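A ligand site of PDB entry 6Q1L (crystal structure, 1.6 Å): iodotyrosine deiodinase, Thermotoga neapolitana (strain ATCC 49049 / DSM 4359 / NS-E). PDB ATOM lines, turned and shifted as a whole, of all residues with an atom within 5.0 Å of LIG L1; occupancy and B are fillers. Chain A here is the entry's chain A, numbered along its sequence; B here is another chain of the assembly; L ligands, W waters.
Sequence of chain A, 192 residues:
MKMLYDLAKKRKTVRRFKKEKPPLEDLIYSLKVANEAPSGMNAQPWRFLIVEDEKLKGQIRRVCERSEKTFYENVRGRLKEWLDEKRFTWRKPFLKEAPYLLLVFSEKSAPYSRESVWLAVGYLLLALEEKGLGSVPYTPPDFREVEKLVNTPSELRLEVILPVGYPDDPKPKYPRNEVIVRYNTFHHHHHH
An oxygen (O3) of LG2 L2 is in hydrogen-bond range of an oxygen (O1) of LIG L1.
The side-chain amino group (NZ) of Lys 92 lies within hydrogen-bond range of the backbone carbonyl oxygen (O) of Thr 89 (2.6 Å). The backbone carbonyl oxygen (O) of Leu 83 is in hydrogen-bond range of the backbone NH (N) of Phe 88 (3.0 Å). O of Met 41 of chain B lies within hydrogen-bond range of NE1 of Trp 82, 3.1 Å away. The side-chain hydroxyl of Tyr 138 lies within hydrogen-bond range of the side-chain carboxylate of Glu 68 (2.7 Å).
The backbone NH (N) of Met 41 of chain B is in hydrogen-bond range of an oxygen (O1) of LIG L1 (2.9 Å). The side-chain amino group (NZ) of Lys 92 is in salt-bridge range of an oxygen (O2) of LIG L1 (2.6 Å). An oxygen (O4) of LG2 L2 sits close to the backbone carbonyl oxygen (O) of Ser 39 of chain B, at 3.4 Å. N of Ser 39 of chain B lies within hydrogen-bond range of O4 of LG2 L2, 3.4 Å away. The side-chain carboxylate (OE2) of Glu 68 is in salt-bridge range of a nitrogen (N1) of LIG L1 (2.8 Å). The guanidinium group of Arg 15 sits at hydrogen-bond distance from an oxygen (O1) of LG2 L2, 2.8 Å away. OH of Tyr 72 is in hydrogen-bond range of O2 of LIG L1. N3 of LG2 L2 sits at hydrogen-bond distance from OG1 of Thr 139 (3.0 Å). The backbone NH of Thr 139 lies within hydrogen-bond range of an oxygen (O2) of LG2 L2 (3.1 Å). The backbone carbonyl oxygen (O) of Thr 139 sits at hydrogen-bond distance from a nitrogen (N1) of LIG L1, 3.4 Å away.
Phe 71 touches LIG L1. Trp 82 touches LIG L1 (CZ3 to C7, 3.7 Å). CD2 of Leu 83 touches C8 of LIG L1, at 3.5 Å. Phe 88 touches LIG L1. Thr 89 touches LIG L1. Tyr 138 touches LIG L1. Gly 40 of chain B touches LIG L1. Pro 111 of chain B touches LIG L1. 13 residues have an atom within 4 Å of LIG L1: Glu 68, Phe 71, Tyr 72, Trp 82, Leu 83, Phe 88, Thr 89, Lys 92, Tyr 138, Thr 139, Gly 40 of chain B, Met 41 of chain B and Pro 111 of chain B. Along chain A the residues within 4 Å of LIG L1 span positions 68 to 139. The nearest printed residue that does not touch LIG L1 is Tyr 112 of chain B (4.2 Å).
Water W3 bridges the side-chain carboxylate of Glu 68 and a nitrogen (N1) of LIG L1. Water W2 lies within hydrogen-bond range of the backbone carbonyl oxygen (O) of Thr 139 (2.6 Å) and a nitrogen (N1) of LIG L1 (3.4 Å). Water W1 lies within hydrogen-bond range of O1 of LG2 L2 (2.7 Å), NZ of Lys 92 (2.9 Å) and O3 of LIG L1 (3.4 Å).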
ATOM      1  N   ARG A  15     -10.216  -4.283 -12.617  1.00  0.00           N
ATOM      2  CA  ARG A  15     -11.053  -4.823 -13.662  1.00  0.00           C
ATOM      3  C   ARG A  15     -10.722  -6.288 -13.942  1.00  0.00           C
ATOM      4  O   ARG A  15     -11.342  -6.889 -14.824  1.00  0.00           O
ATOM      5  CB  ARG A  15     -10.920  -4.015 -14.950  1.00  0.00           C
ATOM      6  CG  ARG A  15     -11.339  -2.563 -14.769  1.00  0.00           C
ATOM      7  CD  ARG A  15     -11.206  -1.782 -16.032  1.00  0.00           C
ATOM      8  NE  ARG A  15     -11.578  -0.372 -15.885  1.00  0.00           N
ATOM      9  CZ  ARG A  15     -10.774   0.618 -15.553  1.00  0.00           C
ATOM     10  NH1 ARG A  15      -9.461   0.416 -15.302  1.00  0.00           N
ATOM     11  NH2 ARG A  15     -11.280   1.843 -15.475  1.00  0.00           N
ATOM     12  N   GLU A  68     -22.516  -0.784 -24.583  1.00  0.00           N
ATOM     13  CA  GLU A  68     -21.158  -0.270 -24.732  1.00  0.00           C
ATOM     14  C   GLU A  68     -20.717  -0.330 -26.185  1.00  0.00           C
ATOM     15  O   GLU A  68     -20.080   0.597 -26.697  1.00  0.00           O
ATOM     16  CB  GLU A  68     -20.175  -1.066 -23.886  1.00  0.00           C
ATOM     17  CG  GLU A  68     -20.335  -0.957 -22.398  1.00  0.00           C
ATOM     18  CD  GLU A  68     -19.975   0.409 -21.878  1.00  0.00           C
ATOM     19  OE1 GLU A  68     -19.778   1.328 -22.708  1.00  0.00           O
ATOM     20  OE2 GLU A  68     -19.896   0.555 -20.629  1.00  0.00           O
ATOM     21  N   PHE A  71     -21.981   2.461 -27.850  1.00  0.00           N
ATOM     22  CA  PHE A  71     -21.314   3.637 -27.309  1.00  0.00           C
ATOM     23  C   PHE A  71     -19.941   3.796 -27.944  1.00  0.00           C
ATOM     24  O   PHE A  71     -19.578   4.892 -28.401  1.00  0.00           O
ATOM     25  CB  PHE A  71     -21.222   3.517 -25.793  1.00  0.00           C
ATOM     26  CG  PHE A  71     -20.285   4.469 -25.159  1.00  0.00           C
ATOM     27  CD1 PHE A  71     -20.686   5.739 -24.805  1.00  0.00           C
ATOM     28  CD2 PHE A  71     -18.973   4.103 -24.932  1.00  0.00           C
ATOM     29  CE1 PHE A  71     -19.798   6.624 -24.224  1.00  0.00           C
ATOM     30  CE2 PHE A  71     -18.096   4.976 -24.336  1.00  0.00           C
ATOM     31  CZ  PHE A  71     -18.506   6.252 -23.991  1.00  0.00           C
ATOM     32  N   TYR A  72     -19.173   2.719 -28.000  1.00  0.00           N
ATOM     33  CA  TYR A  72     -17.830   2.803 -28.566  1.00  0.00           C
ATOM     34  C   TYR A  72     -17.872   3.137 -30.051  1.00  0.00           C
ATOM     35  O   TYR A  72     -16.919   3.724 -30.567  1.00  0.00           O
ATOM     36  CB  TYR A  72     -17.079   1.497 -28.318  1.00  0.00           C
ATOM     37  CG  TYR A  72     -16.367   1.522 -26.991  1.00  0.00           C
ATOM     38  CD1 TYR A  72     -17.057   1.205 -25.839  1.00  0.00           C
ATOM     39  CD2 TYR A  72     -15.052   1.908 -26.886  1.00  0.00           C
ATOM     40  CE1 TYR A  72     -16.432   1.257 -24.629  1.00  0.00           C
ATOM     41  CE2 TYR A  72     -14.416   1.953 -25.682  1.00  0.00           C
ATOM     42  CZ  TYR A  72     -15.128   1.615 -24.544  1.00  0.00           C
ATOM     43  OH  TYR A  72     -14.482   1.694 -23.350  1.00  0.00           O
ATOM     44  N   LEU A  79     -13.571  11.913 -24.029  1.00  0.00           N
ATOM     45  CA  LEU A  79     -13.727  10.559 -23.495  1.00  0.00           C
ATOM     46  C   LEU A  79     -13.235   9.532 -24.518  1.00  0.00           C
ATOM     47  O   LEU A  79     -12.459   8.631 -24.194  1.00  0.00           O
ATOM     48  CB  LEU A  79     -15.173  10.299 -23.083  1.00  0.00           C
ATOM     49  CG  LEU A  79     -15.390   8.962 -22.357  1.00  0.00           C
ATOM     50  CD1 LEU A  79     -14.450   8.766 -21.176  1.00  0.00           C
ATOM     51  CD2 LEU A  79     -16.843   8.886 -21.910  1.00  0.00           C
ATOM     52  N   TRP A  82      -9.491   9.467 -24.424  1.00  0.00           N
ATOM     53  CA  TRP A  82      -8.980   8.789 -23.256  1.00  0.00           C
ATOM     54  C   TRP A  82      -9.176   7.277 -23.344  1.00  0.00           C
ATOM     55  O   TRP A  82      -8.256   6.506 -23.057  1.00  0.00           O
ATOM     56  CB  TRP A  82      -9.685   9.368 -22.015  1.00  0.00           C
ATOM     57  CG  TRP A  82      -9.175   8.909 -20.736  1.00  0.00           C
ATOM     58  CD1 TRP A  82      -8.165   9.451 -20.012  1.00  0.00           C
ATOM     59  CD2 TRP A  82      -9.695   7.828 -19.953  1.00  0.00           C
ATOM     60  NE1 TRP A  82      -8.006   8.770 -18.840  1.00  0.00           N
ATOM     61  CE2 TRP A  82      -8.936   7.762 -18.775  1.00  0.00           C
ATOM     62  CE3 TRP A  82     -10.721   6.911 -20.135  1.00  0.00           C
ATOM     63  CZ2 TRP A  82      -9.159   6.826 -17.780  1.00  0.00           C
ATOM     64  CZ3 TRP A  82     -10.953   5.961 -19.140  1.00  0.00           C
ATOM     65  CH2 TRP A  82     -10.168   5.932 -17.985  1.00  0.00           C
ATOM     66  N   LEU A  83     -10.370   6.852 -23.777  1.00  0.00           N
ATOM     67  CA  LEU A  83     -10.650   5.419 -23.924  1.00  0.00           C
ATOM     68  C   LEU A  83      -9.735   4.786 -24.947  1.00  0.00           C
ATOM     69  O   LEU A  83      -9.264   3.663 -24.753  1.00  0.00           O
ATOM     70  CB  LEU A  83     -12.107   5.199 -24.312  1.00  0.00           C
ATOM     71  CG  LEU A  83     -13.124   5.623 -23.239  1.00  0.00           C
ATOM     72  CD1 LEU A  83     -14.501   5.575 -23.874  1.00  0.00           C
ATOM     73  CD2 LEU A  83     -13.017   4.762 -22.001  1.00  0.00           C
ATOM     74  N   PHE A  88      -9.298   0.770 -23.997  1.00  0.00           N
ATOM     75  CA  PHE A  88     -10.582   0.239 -23.561  1.00  0.00           C
ATOM     76  C   PHE A  88     -11.386  -0.289 -24.746  1.00  0.00           C
ATOM     77  O   PHE A  88     -11.273   0.194 -25.877  1.00  0.00           O
ATOM     78  CB  PHE A  88     -11.412   1.313 -22.866  1.00  0.00           C
ATOM     79  CG  PHE A  88     -11.015   1.618 -21.429  1.00  0.00           C
ATOM     80  CD1 PHE A  88      -9.813   2.208 -21.128  1.00  0.00           C
ATOM     81  CD2 PHE A  88     -11.902   1.407 -20.407  1.00  0.00           C
ATOM     82  CE1 PHE A  88      -9.482   2.525 -19.819  1.00  0.00           C
ATOM     83  CE2 PHE A  88     -11.565   1.727 -19.090  1.00  0.00           C
ATOM     84  CZ  PHE A  88     -10.357   2.262 -18.812  1.00  0.00           C
ATOM     85  N   THR A  89     -12.225  -1.288 -24.473  1.00  0.00           N
ATOM     86  CA  THR A  89     -13.179  -1.756 -25.479  1.00  0.00           C
ATOM     87  C   THR A  89     -14.527  -2.010 -24.823  1.00  0.00           C
ATOM     88  O   THR A  89     -14.699  -1.891 -23.602  1.00  0.00           O
ATOM     89  CB  THR A  89     -12.702  -3.045 -26.145  1.00  0.00           C
ATOM     90  OG1 THR A  89     -12.809  -4.109 -25.204  1.00  0.00           O
ATOM     91  CG2 THR A  89     -11.267  -2.899 -26.580  1.00  0.00           C
ATOM     92  N   LYS A  92     -16.823  -6.532 -21.579  1.00  0.00           N
ATOM     93  CA  LYS A  92     -16.792  -6.341 -20.133  1.00  0.00           C
ATOM     94  C   LYS A  92     -16.731  -7.693 -19.437  1.00  0.00           C
ATOM     95  O   LYS A  92     -17.666  -8.084 -18.721  1.00  0.00           O
ATOM     96  CB  LYS A  92     -18.009  -5.540 -19.658  1.00  0.00           C
ATOM     97  CG  LYS A  92     -18.084  -4.129 -20.205  1.00  0.00           C
ATOM     98  CD  LYS A  92     -16.804  -3.300 -19.989  1.00  0.00           C
ATOM     99  CE  LYS A  92     -16.698  -2.219 -21.033  1.00  0.00           C
ATOM    100  NZ  LYS A  92     -15.330  -1.623 -21.075  1.00  0.00           N
ATOM    101  N   TYR A 138     -18.625   0.769 -12.332  1.00  0.00           N
ATOM    102  CA  TYR A 138     -18.972   0.551 -13.726  1.00  0.00           C
ATOM    103  C   TYR A 138     -20.301   1.231 -14.033  1.00  0.00           C
ATOM    104  O   TYR A 138     -21.294   1.009 -13.341  1.00  0.00           O
ATOM    105  CB  TYR A 138     -19.034  -0.946 -14.025  1.00  0.00           C
ATOM    106  CG  TYR A 138     -19.484  -1.147 -15.422  1.00  0.00           C
ATOM    107  CD1 TYR A 138     -18.755  -0.613 -16.496  1.00  0.00           C
ATOM    108  CD2 TYR A 138     -20.636  -1.843 -15.692  1.00  0.00           C
ATOM    109  CE1 TYR A 138     -19.187  -0.757 -17.770  1.00  0.00           C
ATOM    110  CE2 TYR A 138     -21.089  -1.987 -16.989  1.00  0.00           C
ATOM    111  CZ  TYR A 138     -20.353  -1.456 -18.025  1.00  0.00           C
ATOM    112  OH  TYR A 138     -20.793  -1.595 -19.322  1.00  0.00           O
ATOM    113  N   THR A 139     -20.298   2.088 -15.046  1.00  0.00           N
ATOM    114  CA  THR A 139     -21.461   2.880 -15.415  1.00  0.00           C
ATOM    115  C   THR A 139     -21.741   2.653 -16.887  1.00  0.00           C
ATOM    116  O   THR A 139     -21.199   3.367 -17.748  1.00  0.00           O
ATOM    117  CB  THR A 139     -21.267   4.362 -15.095  1.00  0.00           C
ATOM    118  OG1 THR A 139     -20.085   4.829 -15.733  1.00  0.00           O
ATOM    119  CG2 THR A 139     -21.165   4.597 -13.590  1.00  0.00           C
ATOM    120  N   PRO A 140     -22.573   1.683 -17.231  1.00  0.00           N
ATOM    121  CA  PRO A 140     -22.882   1.402 -18.642  1.00  0.00           C
ATOM    122  C   PRO A 140     -23.753   2.500 -19.220  1.00  0.00           C
ATOM    123  O   PRO A 140     -24.396   3.252 -18.472  1.00  0.00           O
ATOM    124  CB  PRO A 140     -23.653   0.074 -18.583  1.00  0.00           C
ATOM    125  CG  PRO A 140     -24.409   0.189 -17.250  1.00  0.00           C
ATOM    126  CD  PRO A 140     -23.389   0.863 -16.305  1.00  0.00           C
ATOM    127  N   SER B  39     -12.342   8.674 -10.380  1.00  0.00           N
ATOM    128  CA  SER B  39     -13.246   9.601 -11.034  1.00  0.00           C
ATOM    129  C   SER B  39     -13.465   9.134 -12.466  1.00  0.00           C
ATOM    130  O   SER B  39     -12.644   8.406 -13.029  1.00  0.00           O
ATOM    131  CB  SER B  39     -12.699  11.038 -10.984  1.00  0.00           C
ATOM    132  OG  SER B  39     -11.456  11.131 -11.688  1.00  0.00           O
ATOM    133  N   GLY B  40     -14.555   9.601 -13.041  1.00  0.00           N
ATOM    134  CA  GLY B  40     -14.859   9.261 -14.417  1.00  0.00           C
ATOM    135  C   GLY B  40     -13.716   9.722 -15.293  1.00  0.00           C
ATOM    136  O   GLY B  40     -13.284  10.861 -15.184  1.00  0.00           O
ATOM    137  N   MET B  41     -13.176   8.828 -16.113  1.00  0.00           N
ATOM    138  CA  MET B  41     -12.104   9.180 -17.049  1.00  0.00           C
ATOM    139  C   MET B  41     -10.850   9.668 -16.325  1.00  0.00           C
ATOM    140  O   MET B  41      -9.958  10.272 -16.948  1.00  0.00           O
ATOM    141  CB  MET B  41     -12.619  10.262 -18.006  1.00  0.00           C
ATOM    142  CG  MET B  41     -11.870  10.473 -19.283  1.00  0.00           C
ATOM    143  SD  MET B  41     -12.652  11.887 -20.110  1.00  0.00           S
ATOM    144  CE  MET B  41     -11.196  12.630 -20.819  1.00  0.00           C
ATOM    145  N   ASN B  42     -10.734   9.365 -15.021  1.00  0.00           N
ATOM    146  CA  ASN B  42      -9.661   9.903 -14.184  1.00  0.00           C
ATOM    147  C   ASN B  42      -9.537  11.404 -14.373  1.00  0.00           C
ATOM    148  O   ASN B  42      -8.432  11.970 -14.365  1.00  0.00           O
ATOM    149  CB  ASN B  42      -8.305   9.233 -14.461  1.00  0.00           C
ATOM    150  CG  ASN B  42      -7.291   9.499 -13.362  1.00  0.00           C
ATOM    151  OD1 ASN B  42      -7.647   9.633 -12.188  1.00  0.00           O
ATOM    152  ND2 ASN B  42      -6.036   9.572 -13.727  1.00  0.00           N
ATOM    153  N   PRO B 111     -16.927  13.634 -17.673  1.00  0.00           N
ATOM    154  CA  PRO B 111     -17.930  12.569 -17.536  1.00  0.00           C
ATOM    155  C   PRO B 111     -18.120  12.171 -16.079  1.00  0.00           C
ATOM    156  O   PRO B 111     -17.151  11.962 -15.351  1.00  0.00           O
ATOM    157  CB  PRO B 111     -17.321  11.412 -18.341  1.00  0.00           C
ATOM    158  CG  PRO B 111     -16.323  12.054 -19.245  1.00  0.00           C
ATOM    159  CD  PRO B 111     -15.777  13.199 -18.482  1.00  0.00           C
ATOM    160  N   TYR B 112     -19.386  12.060 -15.661  1.00  0.00           N
ATOM    161  CA  TYR B 112     -19.701  11.628 -14.289  1.00  0.00           C
ATOM    162  C   TYR B 112     -19.000  12.532 -13.278  1.00  0.00           C
ATOM    163  O   TYR B 112     -18.589  12.107 -12.191  1.00  0.00           O
ATOM    164  CB  TYR B 112     -19.348  10.157 -14.081  1.00  0.00           C
ATOM    165  CG  TYR B 112     -20.460   9.253 -14.552  1.00  0.00           C
ATOM    166  CD1 TYR B 112     -20.552   8.857 -15.873  1.00  0.00           C
ATOM    167  CD2 TYR B 112     -21.454   8.835 -13.666  1.00  0.00           C
ATOM    168  CE1 TYR B 112     -21.598   8.056 -16.306  1.00  0.00           C
ATOM    169  CE2 TYR B 112     -22.485   8.031 -14.083  1.00  0.00           C
ATOM    170  CZ  TYR B 112     -22.554   7.653 -15.404  1.00  0.00           C
ATOM    171  OH  TYR B 112     -23.597   6.845 -15.822  1.00  0.00           O
HETATM  172  N1  LIG L   1     -18.418   2.653 -19.583  1.00  0.00           N
HETATM  173  C1  LIG L   1     -17.436   2.560 -20.647  1.00  0.00           C
HETATM  174  C2  LIG L   1     -16.597   3.841 -20.824  1.00  0.00           C
HETATM  175  C3  LIG L   1     -15.940   4.396 -19.612  1.00  0.00           C
HETATM  176  C4  LIG L   1     -16.456   5.534 -19.011  1.00  0.00           C
HETATM  177  C5  LIG L   1     -15.827   6.096 -17.902  1.00  0.00           C
HETATM  178  I1  LIG L   1     -16.720   7.691 -17.081  1.00  0.00           I
HETATM  179  C6  LIG L   1     -14.673   5.545 -17.397  1.00  0.00           C
HETATM  180  O1  LIG L   1     -14.009   6.039 -16.328  1.00  0.00           O
HETATM  181  C7  LIG L   1     -14.126   4.407 -17.996  1.00  0.00           C
HETATM  182  C8  LIG L   1     -14.756   3.845 -19.104  1.00  0.00           C
HETATM  183  C9  LIG L   1     -16.491   1.406 -20.407  1.00  0.00           C
HETATM  184  O2  LIG L   1     -15.620   0.994 -21.201  1.00  0.00           O
HETATM  185  O3  LIG L   1     -16.562   0.798 -19.214  1.00  0.00           O
HETATM  186  N1  LG2 L   2     -14.268   2.462 -15.256  1.00  0.00           N
HETATM  187  C1  LG2 L   2     -14.677   1.694 -16.321  1.00  0.00           C
HETATM  188  O1  LG2 L   2     -13.934   0.856 -16.800  1.00  0.00           O
HETATM  189  N2  LG2 L   2     -15.929   1.847 -16.832  1.00  0.00           N
HETATM  190  C2  LG2 L   2     -16.815   2.752 -16.360  1.00  0.00           C
HETATM  191  O2  LG2 L   2     -17.929   2.833 -16.886  1.00  0.00           O
HETATM  192  C3  LG2 L   2     -16.396   3.534 -15.296  1.00  0.00           C
HETATM  193  N3  LG2 L   2     -17.253   4.477 -14.782  1.00  0.00           N
HETATM  194  C4  LG2 L   2     -16.865   5.218 -13.702  1.00  0.00           C
HETATM  195  C5  LG2 L   2     -17.776   6.144 -13.177  1.00  0.00           C
HETATM  196  C6  LG2 L   2     -17.414   6.912 -12.074  1.00  0.00           C
HETATM  197  C7  LG2 L   2     -18.404   7.904 -11.485  1.00  0.00           C
HETATM  198  C8  LG2 L   2     -16.129   6.767 -11.511  1.00  0.00           C
HETATM  199  C9  LG2 L   2     -15.707   7.582 -10.300  1.00  0.00           C
HETATM  200  C10 LG2 L   2     -15.224   5.838 -12.043  1.00  0.00           C
HETATM  201  C11 LG2 L   2     -15.599   5.086 -13.156  1.00  0.00           C
HETATM  202  N4  LG2 L   2     -14.709   4.160 -13.704  1.00  0.00           N
HETATM  203  C12 LG2 L   2     -15.143   3.375 -14.755  1.00  0.00           C
HETATM  204  C13 LG2 L   2     -13.334   3.976 -13.185  1.00  0.00           C
HETATM  205  C14 LG2 L   2     -12.446   5.144 -13.666  1.00  0.00           C
HETATM  206  O3  LG2 L   2     -12.043   4.897 -14.994  1.00  0.00           O
HETATM  207  C15 LG2 L   2     -11.248   5.186 -12.717  1.00  0.00           C
HETATM  208  O4  LG2 L   2     -11.699   5.529 -11.419  1.00  0.00           O
HETATM  209  C16 LG2 L   2     -10.121   6.135 -13.137  1.00  0.00           C
HETATM  210  O5  LG2 L   2      -9.590   5.639 -14.354  1.00  0.00           O
HETATM  211  C17 LG2 L   2      -9.039   6.216 -12.082  1.00  0.00           C
HETATM  212  O6  LG2 L   2      -8.471   4.935 -11.819  1.00  0.00           O
HETATM  213  P1  LG2 L   2      -7.346   4.802 -10.721  1.00  0.00           P
HETATM  214  O7  LG2 L   2      -7.002   3.305 -10.890  1.00  0.00           O
HETATM  215  O8  LG2 L   2      -7.862   5.088  -9.372  1.00  0.00           O
HETATM  216  O9  LG2 L   2      -6.179   5.686 -11.172  1.00  0.00           O
HETATM  217  O   HOH W   1     -13.795  -1.132 -18.660  1.00  0.00           O
HETATM  218  O   HOH W   2     -20.019   5.474 -18.710  1.00  0.00           O
HETATM  219  O   HOH W   3     -20.113   4.006 -21.802  1.00  0.00           O
